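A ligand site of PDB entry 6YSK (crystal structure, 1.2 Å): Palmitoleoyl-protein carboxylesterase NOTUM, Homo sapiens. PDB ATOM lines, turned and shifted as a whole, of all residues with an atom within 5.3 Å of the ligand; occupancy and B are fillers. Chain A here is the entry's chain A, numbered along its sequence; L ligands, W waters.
An oxygen (O2) of the ligand is in hydrogen-bond range of the backbone NH of Trp 51, at 2.9 Å. An oxygen (O2) of the ligand lies within hydrogen-bond range of the backbone NH (N) of Ala 156 (2.9 Å). An oxygen (O2) of the ligand is in hydrogen-bond range of the backbone NH of Gly 50 (2.9 Å).
OG of Ser 155 lies within hydrogen-bond range of NE2 of His 312 (3.0 Å). The side-chain hydroxyl of Thr 159 lies within hydrogen-bond range of the backbone carbonyl oxygen of Gly 189, at 2.9 Å. The backbone carbonyl oxygen of Ser 154 sits close to the backbone NH of Gly 49, 3.3 Å away. OH of Tyr 105 sits at hydrogen-bond distance from O of Trp 51 (2.7 Å).
The backbone carbonyl oxygen of Pro 210 lies close to a fluorine (F1) of the ligand, at 3.3 Å. Gly 49 touches the ligand (C to O2, 3.96 Å). CE2 of Tyr 52 touches N1 of the ligand, at 3.5 Å. CB of Ser 155 touches O2 of the ligand, 3.3 Å away. OG1 of Thr 159 touches C10 of the ligand, 3.4 Å away. CB of Phe 191 touches F3 of the ligand (3.1 Å). CG1 of Ile 214 touches F1 of the ligand, 3.2 Å away. Phe 242 touches the ligand (O to CL1, 3.5 Å). Phe 243 touches the ligand. Ala 265 touches the ligand. CG2 of Val 269 touches F2 of the ligand, at 3.7 Å. His 312 touches the ligand (CE1 to O1, 3.3 Å). Hydrophobic or aromatic side chains within 4 Å of the ligand: Trp 51, Tyr 52, Ala 156, Phe 191, Pro 210, Ile 214, Phe 242, Phe 243, Ala 265, Val 269 and His 312. Of the 24 residues printed, 15 come within 4 Å of the ligand. The nearest printed residue that does not touch the ligand is Val 110 (4.2 Å).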
ATOM      1  N   GLY A  49      21.779  -1.601 -19.782  1.00  0.00           N
ATOM      2  CA  GLY A  49      20.360  -1.770 -20.053  1.00  0.00           C
ATOM      3  C   GLY A  49      20.077  -2.044 -21.517  1.00  0.00           C
ATOM      4  O   GLY A  49      20.984  -2.360 -22.277  1.00  0.00           O
ATOM      5  N   GLY A  50      18.792  -1.960 -21.884  1.00  0.00           N
ATOM      6  CA  GLY A  50      18.393  -2.220 -23.269  1.00  0.00           C
ATOM      7  C   GLY A  50      17.153  -3.090 -23.409  1.00  0.00           C
ATOM      8  O   GLY A  50      17.198  -4.130 -24.082  1.00  0.00           O
ATOM      9  N   TRP A  51      16.053  -2.665 -22.801  1.00  0.00           N
ATOM     10  CA  TRP A  51      14.766  -3.355 -22.902  1.00  0.00           C
ATOM     11  C   TRP A  51      14.934  -4.787 -22.374  1.00  0.00           C
ATOM     12  O   TRP A  51      15.576  -4.993 -21.325  1.00  0.00           O
ATOM     13  CB  TRP A  51      14.143  -3.211 -24.304  1.00  0.00           C
ATOM     14  CG  TRP A  51      13.677  -1.781 -24.512  1.00  0.00           C
ATOM     15  CD1 TRP A  51      14.388  -0.772 -25.113  1.00  0.00           C
ATOM     16  CD2 TRP A  51      12.430  -1.199 -24.083  1.00  0.00           C
ATOM     17  NE1 TRP A  51      13.652   0.379 -25.102  1.00  0.00           N
ATOM     18  CE2 TRP A  51      12.445   0.161 -24.480  1.00  0.00           C
ATOM     19  CE3 TRP A  51      11.300  -1.705 -23.450  1.00  0.00           C
ATOM     20  CZ2 TRP A  51      11.381   1.021 -24.244  1.00  0.00           C
ATOM     21  CZ3 TRP A  51      10.235  -0.835 -23.206  1.00  0.00           C
ATOM     22  CH2 TRP A  51      10.297   0.525 -23.597  1.00  0.00           C
ATOM     23  N   TYR A  52      14.251  -5.754 -22.994  1.00  0.00           N
ATOM     24  CA  TYR A  52      14.039  -7.107 -22.510  1.00  0.00           C
ATOM     25  C   TYR A  52      13.176  -7.790 -23.570  1.00  0.00           C
ATOM     26  O   TYR A  52      12.714  -7.137 -24.503  1.00  0.00           O
ATOM     27  CB  TYR A  52      13.300  -7.119 -21.166  1.00  0.00           C
ATOM     28  CG  TYR A  52      12.196  -6.101 -21.005  1.00  0.00           C
ATOM     29  CD1 TYR A  52      10.945  -6.299 -21.554  1.00  0.00           C
ATOM     30  CD2 TYR A  52      12.432  -4.911 -20.310  1.00  0.00           C
ATOM     31  CE1 TYR A  52       9.928  -5.339 -21.393  1.00  0.00           C
ATOM     32  CE2 TYR A  52      11.432  -3.947 -20.163  1.00  0.00           C
ATOM     33  CZ  TYR A  52      10.206  -4.163 -20.710  1.00  0.00           C
ATOM     34  OH  TYR A  52       9.214  -3.214 -20.523  1.00  0.00           O
ATOM     35  N   TYR A 105      24.721  -6.408 -21.102  1.00  0.00           N
ATOM     36  CA  TYR A 105      23.397  -6.994 -20.920  1.00  0.00           C
ATOM     37  C   TYR A 105      23.113  -7.893 -22.103  1.00  0.00           C
ATOM     38  O   TYR A 105      22.906  -7.417 -23.225  1.00  0.00           O
ATOM     39  CB  TYR A 105      22.411  -5.841 -20.887  1.00  0.00           C
ATOM     40  CG  TYR A 105      20.956  -6.169 -20.676  1.00  0.00           C
ATOM     41  CD1 TYR A 105      20.526  -7.115 -19.746  1.00  0.00           C
ATOM     42  CD2 TYR A 105      19.989  -5.442 -21.353  1.00  0.00           C
ATOM     43  CE1 TYR A 105      19.203  -7.320 -19.500  1.00  0.00           C
ATOM     44  CE2 TYR A 105      18.619  -5.636 -21.103  1.00  0.00           C
ATOM     45  CZ  TYR A 105      18.253  -6.588 -20.191  1.00  0.00           C
ATOM     46  OH  TYR A 105      16.927  -6.816 -19.920  1.00  0.00           O
ATOM     47  N   VAL A 110      16.023  -8.182 -17.566  1.00  0.00           N
ATOM     48  CA  VAL A 110      16.116  -7.196 -16.490  1.00  0.00           C
ATOM     49  C   VAL A 110      17.047  -7.703 -15.383  1.00  0.00           C
ATOM     50  O   VAL A 110      16.911  -7.340 -14.212  1.00  0.00           O
ATOM     51  CB  VAL A 110      14.742  -6.718 -15.992  1.00  0.00           C
ATOM     52  CG1 VAL A 110      14.863  -5.371 -15.239  1.00  0.00           C
ATOM     53  CG2 VAL A 110      13.740  -6.581 -17.130  1.00  0.00           C
ATOM     54  N   SER A 154      22.162   1.195 -15.601  1.00  0.00           N
ATOM     55  CA  SER A 154      21.222   2.119 -16.208  1.00  0.00           C
ATOM     56  C   SER A 154      20.074   1.373 -16.868  1.00  0.00           C
ATOM     57  O   SER A 154      20.301   0.366 -17.569  1.00  0.00           O
ATOM     58  CB  SER A 154      21.901   2.951 -17.272  1.00  0.00           C
ATOM     59  OG  SER A 154      22.885   3.813 -16.684  1.00  0.00           O
ATOM     60  N   SER A 155      18.873   1.930 -16.735  1.00  0.00           N
ATOM     61  CA  SER A 155      17.666   1.471 -17.455  1.00  0.00           C
ATOM     62  C   SER A 155      17.366   0.073 -16.941  1.00  0.00           C
ATOM     63  O   SER A 155      17.209  -0.082 -15.726  1.00  0.00           O
ATOM     64  CB  SER A 155      17.829   1.646 -18.956  1.00  0.00           C
ATOM     65  OG  SER A 155      18.406   2.911 -19.305  1.00  0.00           O
ATOM     66  N   ALA A 156      17.285  -0.952 -17.802  1.00  0.00           N
ATOM     67  CA  ALA A 156      17.096  -2.309 -17.269  1.00  0.00           C
ATOM     68  C   ALA A 156      18.200  -2.648 -16.277  1.00  0.00           C
ATOM     69  O   ALA A 156      17.949  -3.366 -15.284  1.00  0.00           O
ATOM     70  CB  ALA A 156      17.049  -3.354 -18.381  1.00  0.00           C
ATOM     71  N   GLY A 157      19.419  -2.121 -16.489  1.00  0.00           N
ATOM     72  CA  GLY A 157      20.474  -2.336 -15.513  1.00  0.00           C
ATOM     73  C   GLY A 157      20.256  -1.618 -14.194  1.00  0.00           C
ATOM     74  O   GLY A 157      20.724  -2.100 -13.153  1.00  0.00           O
ATOM     75  N   THR A 159      17.222  -1.228 -12.799  1.00  0.00           N
ATOM     76  CA  THR A 159      16.354  -2.170 -12.100  1.00  0.00           C
ATOM     77  C   THR A 159      17.154  -3.386 -11.649  1.00  0.00           C
ATOM     78  O   THR A 159      16.920  -3.910 -10.551  1.00  0.00           O
ATOM     79  CB  THR A 159      15.189  -2.562 -12.996  1.00  0.00           C
ATOM     80  OG1 THR A 159      14.573  -1.399 -13.558  1.00  0.00           O
ATOM     81  CG2 THR A 159      14.157  -3.372 -12.206  1.00  0.00           C
ATOM     82  N   GLY A 189      16.028   3.202 -13.523  1.00  0.00           N
ATOM     83  CA  GLY A 189      15.420   1.887 -13.314  1.00  0.00           C
ATOM     84  C   GLY A 189      14.302   1.905 -12.320  1.00  0.00           C
ATOM     85  O   GLY A 189      13.897   0.844 -11.841  1.00  0.00           O
ATOM     86  N   PHE A 191      10.637   2.569 -11.932  1.00  0.00           N
ATOM     87  CA  PHE A 191       9.429   2.653 -12.757  1.00  0.00           C
ATOM     88  C   PHE A 191       8.167   2.648 -11.921  1.00  0.00           C
ATOM     89  O   PHE A 191       8.151   2.146 -10.782  1.00  0.00           O
ATOM     90  CB  PHE A 191       9.397   1.473 -13.760  1.00  0.00           C
ATOM     91  CG  PHE A 191      10.423   1.605 -14.813  1.00  0.00           C
ATOM     92  CD1 PHE A 191      10.167   2.373 -15.917  1.00  0.00           C
ATOM     93  CD2 PHE A 191      11.647   1.019 -14.679  1.00  0.00           C
ATOM     94  CE1 PHE A 191      11.172   2.542 -16.919  1.00  0.00           C
ATOM     95  CE2 PHE A 191      12.625   1.171 -15.655  1.00  0.00           C
ATOM     96  CZ  PHE A 191      12.400   1.931 -16.725  1.00  0.00           C
ATOM     97  N   LEU A 192       7.090   3.168 -12.486  1.00  0.00           N
ATOM     98  CA  LEU A 192       5.778   3.116 -11.869  1.00  0.00           C
ATOM     99  C   LEU A 192       4.919   2.103 -12.615  1.00  0.00           C
ATOM    100  O   LEU A 192       4.883   2.094 -13.859  1.00  0.00           O
ATOM    101  CB  LEU A 192       5.094   4.484 -11.945  1.00  0.00           C
ATOM    102  CG  LEU A 192       5.858   5.621 -11.220  1.00  0.00           C
ATOM    103  CD1 LEU A 192       5.072   6.903 -11.318  1.00  0.00           C
ATOM    104  CD2 LEU A 192       6.163   5.247  -9.755  1.00  0.00           C
ATOM    105  N   PRO A 210       3.433  -1.645 -18.028  1.00  0.00           N
ATOM    106  CA  PRO A 210       4.474  -2.118 -17.106  1.00  0.00           C
ATOM    107  C   PRO A 210       4.110  -3.377 -16.329  1.00  0.00           C
ATOM    108  O   PRO A 210       4.890  -4.328 -16.271  1.00  0.00           O
ATOM    109  CB  PRO A 210       4.661  -0.927 -16.142  1.00  0.00           C
ATOM    110  CG  PRO A 210       4.194   0.229 -16.861  1.00  0.00           C
ATOM    111  CD  PRO A 210       3.149  -0.202 -17.892  1.00  0.00           C
ATOM    112  N   THR A 211       2.900  -3.412 -15.741  1.00  0.00           N
ATOM    113  CA  THR A 211       2.561  -4.567 -14.908  1.00  0.00           C
ATOM    114  C   THR A 211       2.488  -5.834 -15.754  1.00  0.00           C
ATOM    115  O   THR A 211       2.942  -6.903 -15.334  1.00  0.00           O
ATOM    116  CB  THR A 211       1.185  -4.338 -14.280  1.00  0.00           C
ATOM    117  OG1 THR A 211       0.259  -4.033 -15.321  1.00  0.00           O
ATOM    118  CG2 THR A 211       1.219  -3.184 -13.333  1.00  0.00           C
ATOM    119  N   ALA A 213       4.047  -6.430 -18.624  1.00  0.00           N
ATOM    120  CA  ALA A 213       5.344  -6.835 -19.148  1.00  0.00           C
ATOM    121  C   ALA A 213       6.086  -7.656 -18.115  1.00  0.00           C
ATOM    122  O   ALA A 213       6.630  -8.717 -18.425  1.00  0.00           O
ATOM    123  CB  ALA A 213       6.162  -5.610 -19.563  1.00  0.00           C
ATOM    124  N   ILE A 214       6.086  -7.205 -16.858  1.00  0.00           N
ATOM    125  CA  ILE A 214       6.833  -7.902 -15.813  1.00  0.00           C
ATOM    126  C   ILE A 214       6.132  -9.198 -15.402  1.00  0.00           C
ATOM    127  O   ILE A 214       6.805 -10.214 -15.187  1.00  0.00           O
ATOM    128  CB  ILE A 214       7.093  -6.990 -14.606  1.00  0.00           C
ATOM    129  CG1 ILE A 214       7.816  -5.691 -15.060  1.00  0.00           C
ATOM    130  CG2 ILE A 214       7.901  -7.719 -13.541  1.00  0.00           C
ATOM    131  CD1 ILE A 214       9.064  -5.994 -15.916  1.00  0.00           C
ATOM    132  N   PHE A 242       9.919  -5.802  -9.024  1.00  0.00           N
ATOM    133  CA  PHE A 242      10.651  -5.092 -10.064  1.00  0.00           C
ATOM    134  C   PHE A 242      10.425  -3.595  -9.991  1.00  0.00           C
ATOM    135  O   PHE A 242      11.104  -2.845 -10.710  1.00  0.00           O
ATOM    136  CB  PHE A 242      10.201  -5.588 -11.446  1.00  0.00           C
ATOM    137  CG  PHE A 242      10.816  -6.898 -11.876  1.00  0.00           C
ATOM    138  CD1 PHE A 242      10.585  -8.050 -11.161  1.00  0.00           C
ATOM    139  CD2 PHE A 242      11.607  -6.970 -13.015  1.00  0.00           C
ATOM    140  CE1 PHE A 242      11.084  -9.299 -11.596  1.00  0.00           C
ATOM    141  CE2 PHE A 242      12.120  -8.239 -13.426  1.00  0.00           C
ATOM    142  CZ  PHE A 242      11.886  -9.367 -12.706  1.00  0.00           C
ATOM    143  N   PHE A 243       9.468  -3.138  -9.149  1.00  0.00           N
ATOM    144  CA  PHE A 243       9.088  -1.725  -9.074  1.00  0.00           C
ATOM    145  C   PHE A 243       9.819  -1.107  -7.893  1.00  0.00           C
ATOM    146  O   PHE A 243       9.571  -1.494  -6.737  1.00  0.00           O
ATOM    147  CB  PHE A 243       7.570  -1.590  -9.047  1.00  0.00           C
ATOM    148  CG  PHE A 243       7.008  -1.954 -10.376  1.00  0.00           C
ATOM    149  CD1 PHE A 243       6.978  -1.004 -11.392  1.00  0.00           C
ATOM    150  CD2 PHE A 243       6.679  -3.268 -10.668  1.00  0.00           C
ATOM    151  CE1 PHE A 243       6.560  -1.357 -12.687  1.00  0.00           C
ATOM    152  CE2 PHE A 243       6.283  -3.605 -11.946  1.00  0.00           C
ATOM    153  CZ  PHE A 243       6.231  -2.663 -12.955  1.00  0.00           C
ATOM    154  N   ALA A 265      11.524   5.981 -21.252  1.00  0.00           N
ATOM    155  CA  ALA A 265      11.059   4.597 -21.301  1.00  0.00           C
ATOM    156  C   ALA A 265       9.771   4.402 -20.512  1.00  0.00           C
ATOM    157  O   ALA A 265       8.886   3.664 -20.961  1.00  0.00           O
ATOM    158  CB  ALA A 265      12.145   3.655 -20.817  1.00  0.00           C
ATOM    159  N   GLN A 266       9.617   5.097 -19.372  1.00  0.00           N
ATOM    160  CA  GLN A 266       8.347   5.102 -18.665  1.00  0.00           C
ATOM    161  C   GLN A 266       7.232   5.613 -19.563  1.00  0.00           C
ATOM    162  O   GLN A 266       6.170   4.990 -19.672  1.00  0.00           O
ATOM    163  CB  GLN A 266       8.473   5.954 -17.415  1.00  0.00           C
ATOM    164  CG  GLN A 266       7.155   6.097 -16.612  1.00  0.00           C
ATOM    165  CD  GLN A 266       6.878   4.905 -15.731  1.00  0.00           C
ATOM    166  OE1 GLN A 266       7.690   4.501 -14.931  1.00  0.00           O
ATOM    167  NE2 GLN A 266       5.693   4.341 -15.918  1.00  0.00           N
ATOM    168  N   VAL A 269       6.339   2.903 -22.294  1.00  0.00           N
ATOM    169  CA  VAL A 269       5.471   1.822 -21.811  1.00  0.00           C
ATOM    170  C   VAL A 269       4.091   2.337 -21.427  1.00  0.00           C
ATOM    171  O   VAL A 269       3.133   1.569 -21.397  1.00  0.00           O
ATOM    172  CB  VAL A 269       6.102   0.961 -20.681  1.00  0.00           C
ATOM    173  CG1 VAL A 269       7.386   0.292 -21.180  1.00  0.00           C
ATOM    174  CG2 VAL A 269       6.361   1.770 -19.444  1.00  0.00           C
ATOM    175  N   HIS A 312      16.562   9.978 -21.077  1.00  0.00           N
ATOM    176  CA  HIS A 312      16.777   8.575 -20.726  1.00  0.00           C
ATOM    177  C   HIS A 312      18.240   8.334 -20.397  1.00  0.00           C
ATOM    178  O   HIS A 312      19.108   8.611 -21.228  1.00  0.00           O
ATOM    179  CB  HIS A 312      16.358   7.642 -21.874  1.00  0.00           C
ATOM    180  CG  HIS A 312      16.312   6.187 -21.481  1.00  0.00           C
ATOM    181  ND1 HIS A 312      16.884   5.204 -22.247  1.00  0.00           N
ATOM    182  CD2 HIS A 312      15.774   5.572 -20.400  1.00  0.00           C
ATOM    183  CE1 HIS A 312      16.706   4.033 -21.653  1.00  0.00           C
ATOM    184  NE2 HIS A 312      16.035   4.231 -20.535  1.00  0.00           N
HETATM  185  C1  LIG L   1      12.672  -1.916 -16.703  1.00  0.00           C
HETATM  186  C2  LIG L   1       9.927  -1.640 -16.549  1.00  0.00           C
HETATM  187  C3  LIG L   1       8.410  -1.508 -16.508  1.00  0.00           C
HETATM  188  C4  LIG L   1      15.593   0.019 -20.862  1.00  0.00           C
HETATM  189  C5  LIG L   1      14.198   0.276 -20.141  1.00  0.00           C
HETATM  190  C6  LIG L   1      13.135   0.082 -20.971  1.00  0.00           C
HETATM  191  C7  LIG L   1      11.920  -0.233 -19.913  1.00  0.00           C
HETATM  192  C8  LIG L   1      14.091  -0.734 -18.924  1.00  0.00           C
HETATM  193  C9  LIG L   1      11.918  -1.368 -17.721  1.00  0.00           C
HETATM  194  C10 LIG L   1      12.023  -2.308 -15.542  1.00  0.00           C
HETATM  195  C11 LIG L   1      10.634  -2.176 -15.476  1.00  0.00           C
HETATM  196  C12 LIG L   1      10.553  -1.246 -17.694  1.00  0.00           C
HETATM  197  F1  LIG L   1       7.802  -2.707 -16.268  1.00  0.00           F
HETATM  198  F2  LIG L   1       7.928  -1.073 -17.688  1.00  0.00           F
HETATM  199  F3  LIG L   1       8.029  -0.655 -15.566  1.00  0.00           F
HETATM  200  N1  LIG L   1      12.596  -0.924 -18.937  1.00  0.00           N
HETATM  201  O1  LIG L   1      15.810   0.901 -21.755  1.00  0.00           O
HETATM  202  O2  LIG L   1      16.410  -0.870 -20.582  1.00  0.00           O
HETATM  203 CL1  LIG L   1       9.848  -2.660 -13.983  1.00  0.00          CL
HETATM  204  O   HOH W   1      18.025   1.300 -22.958  1.00  0.00           O
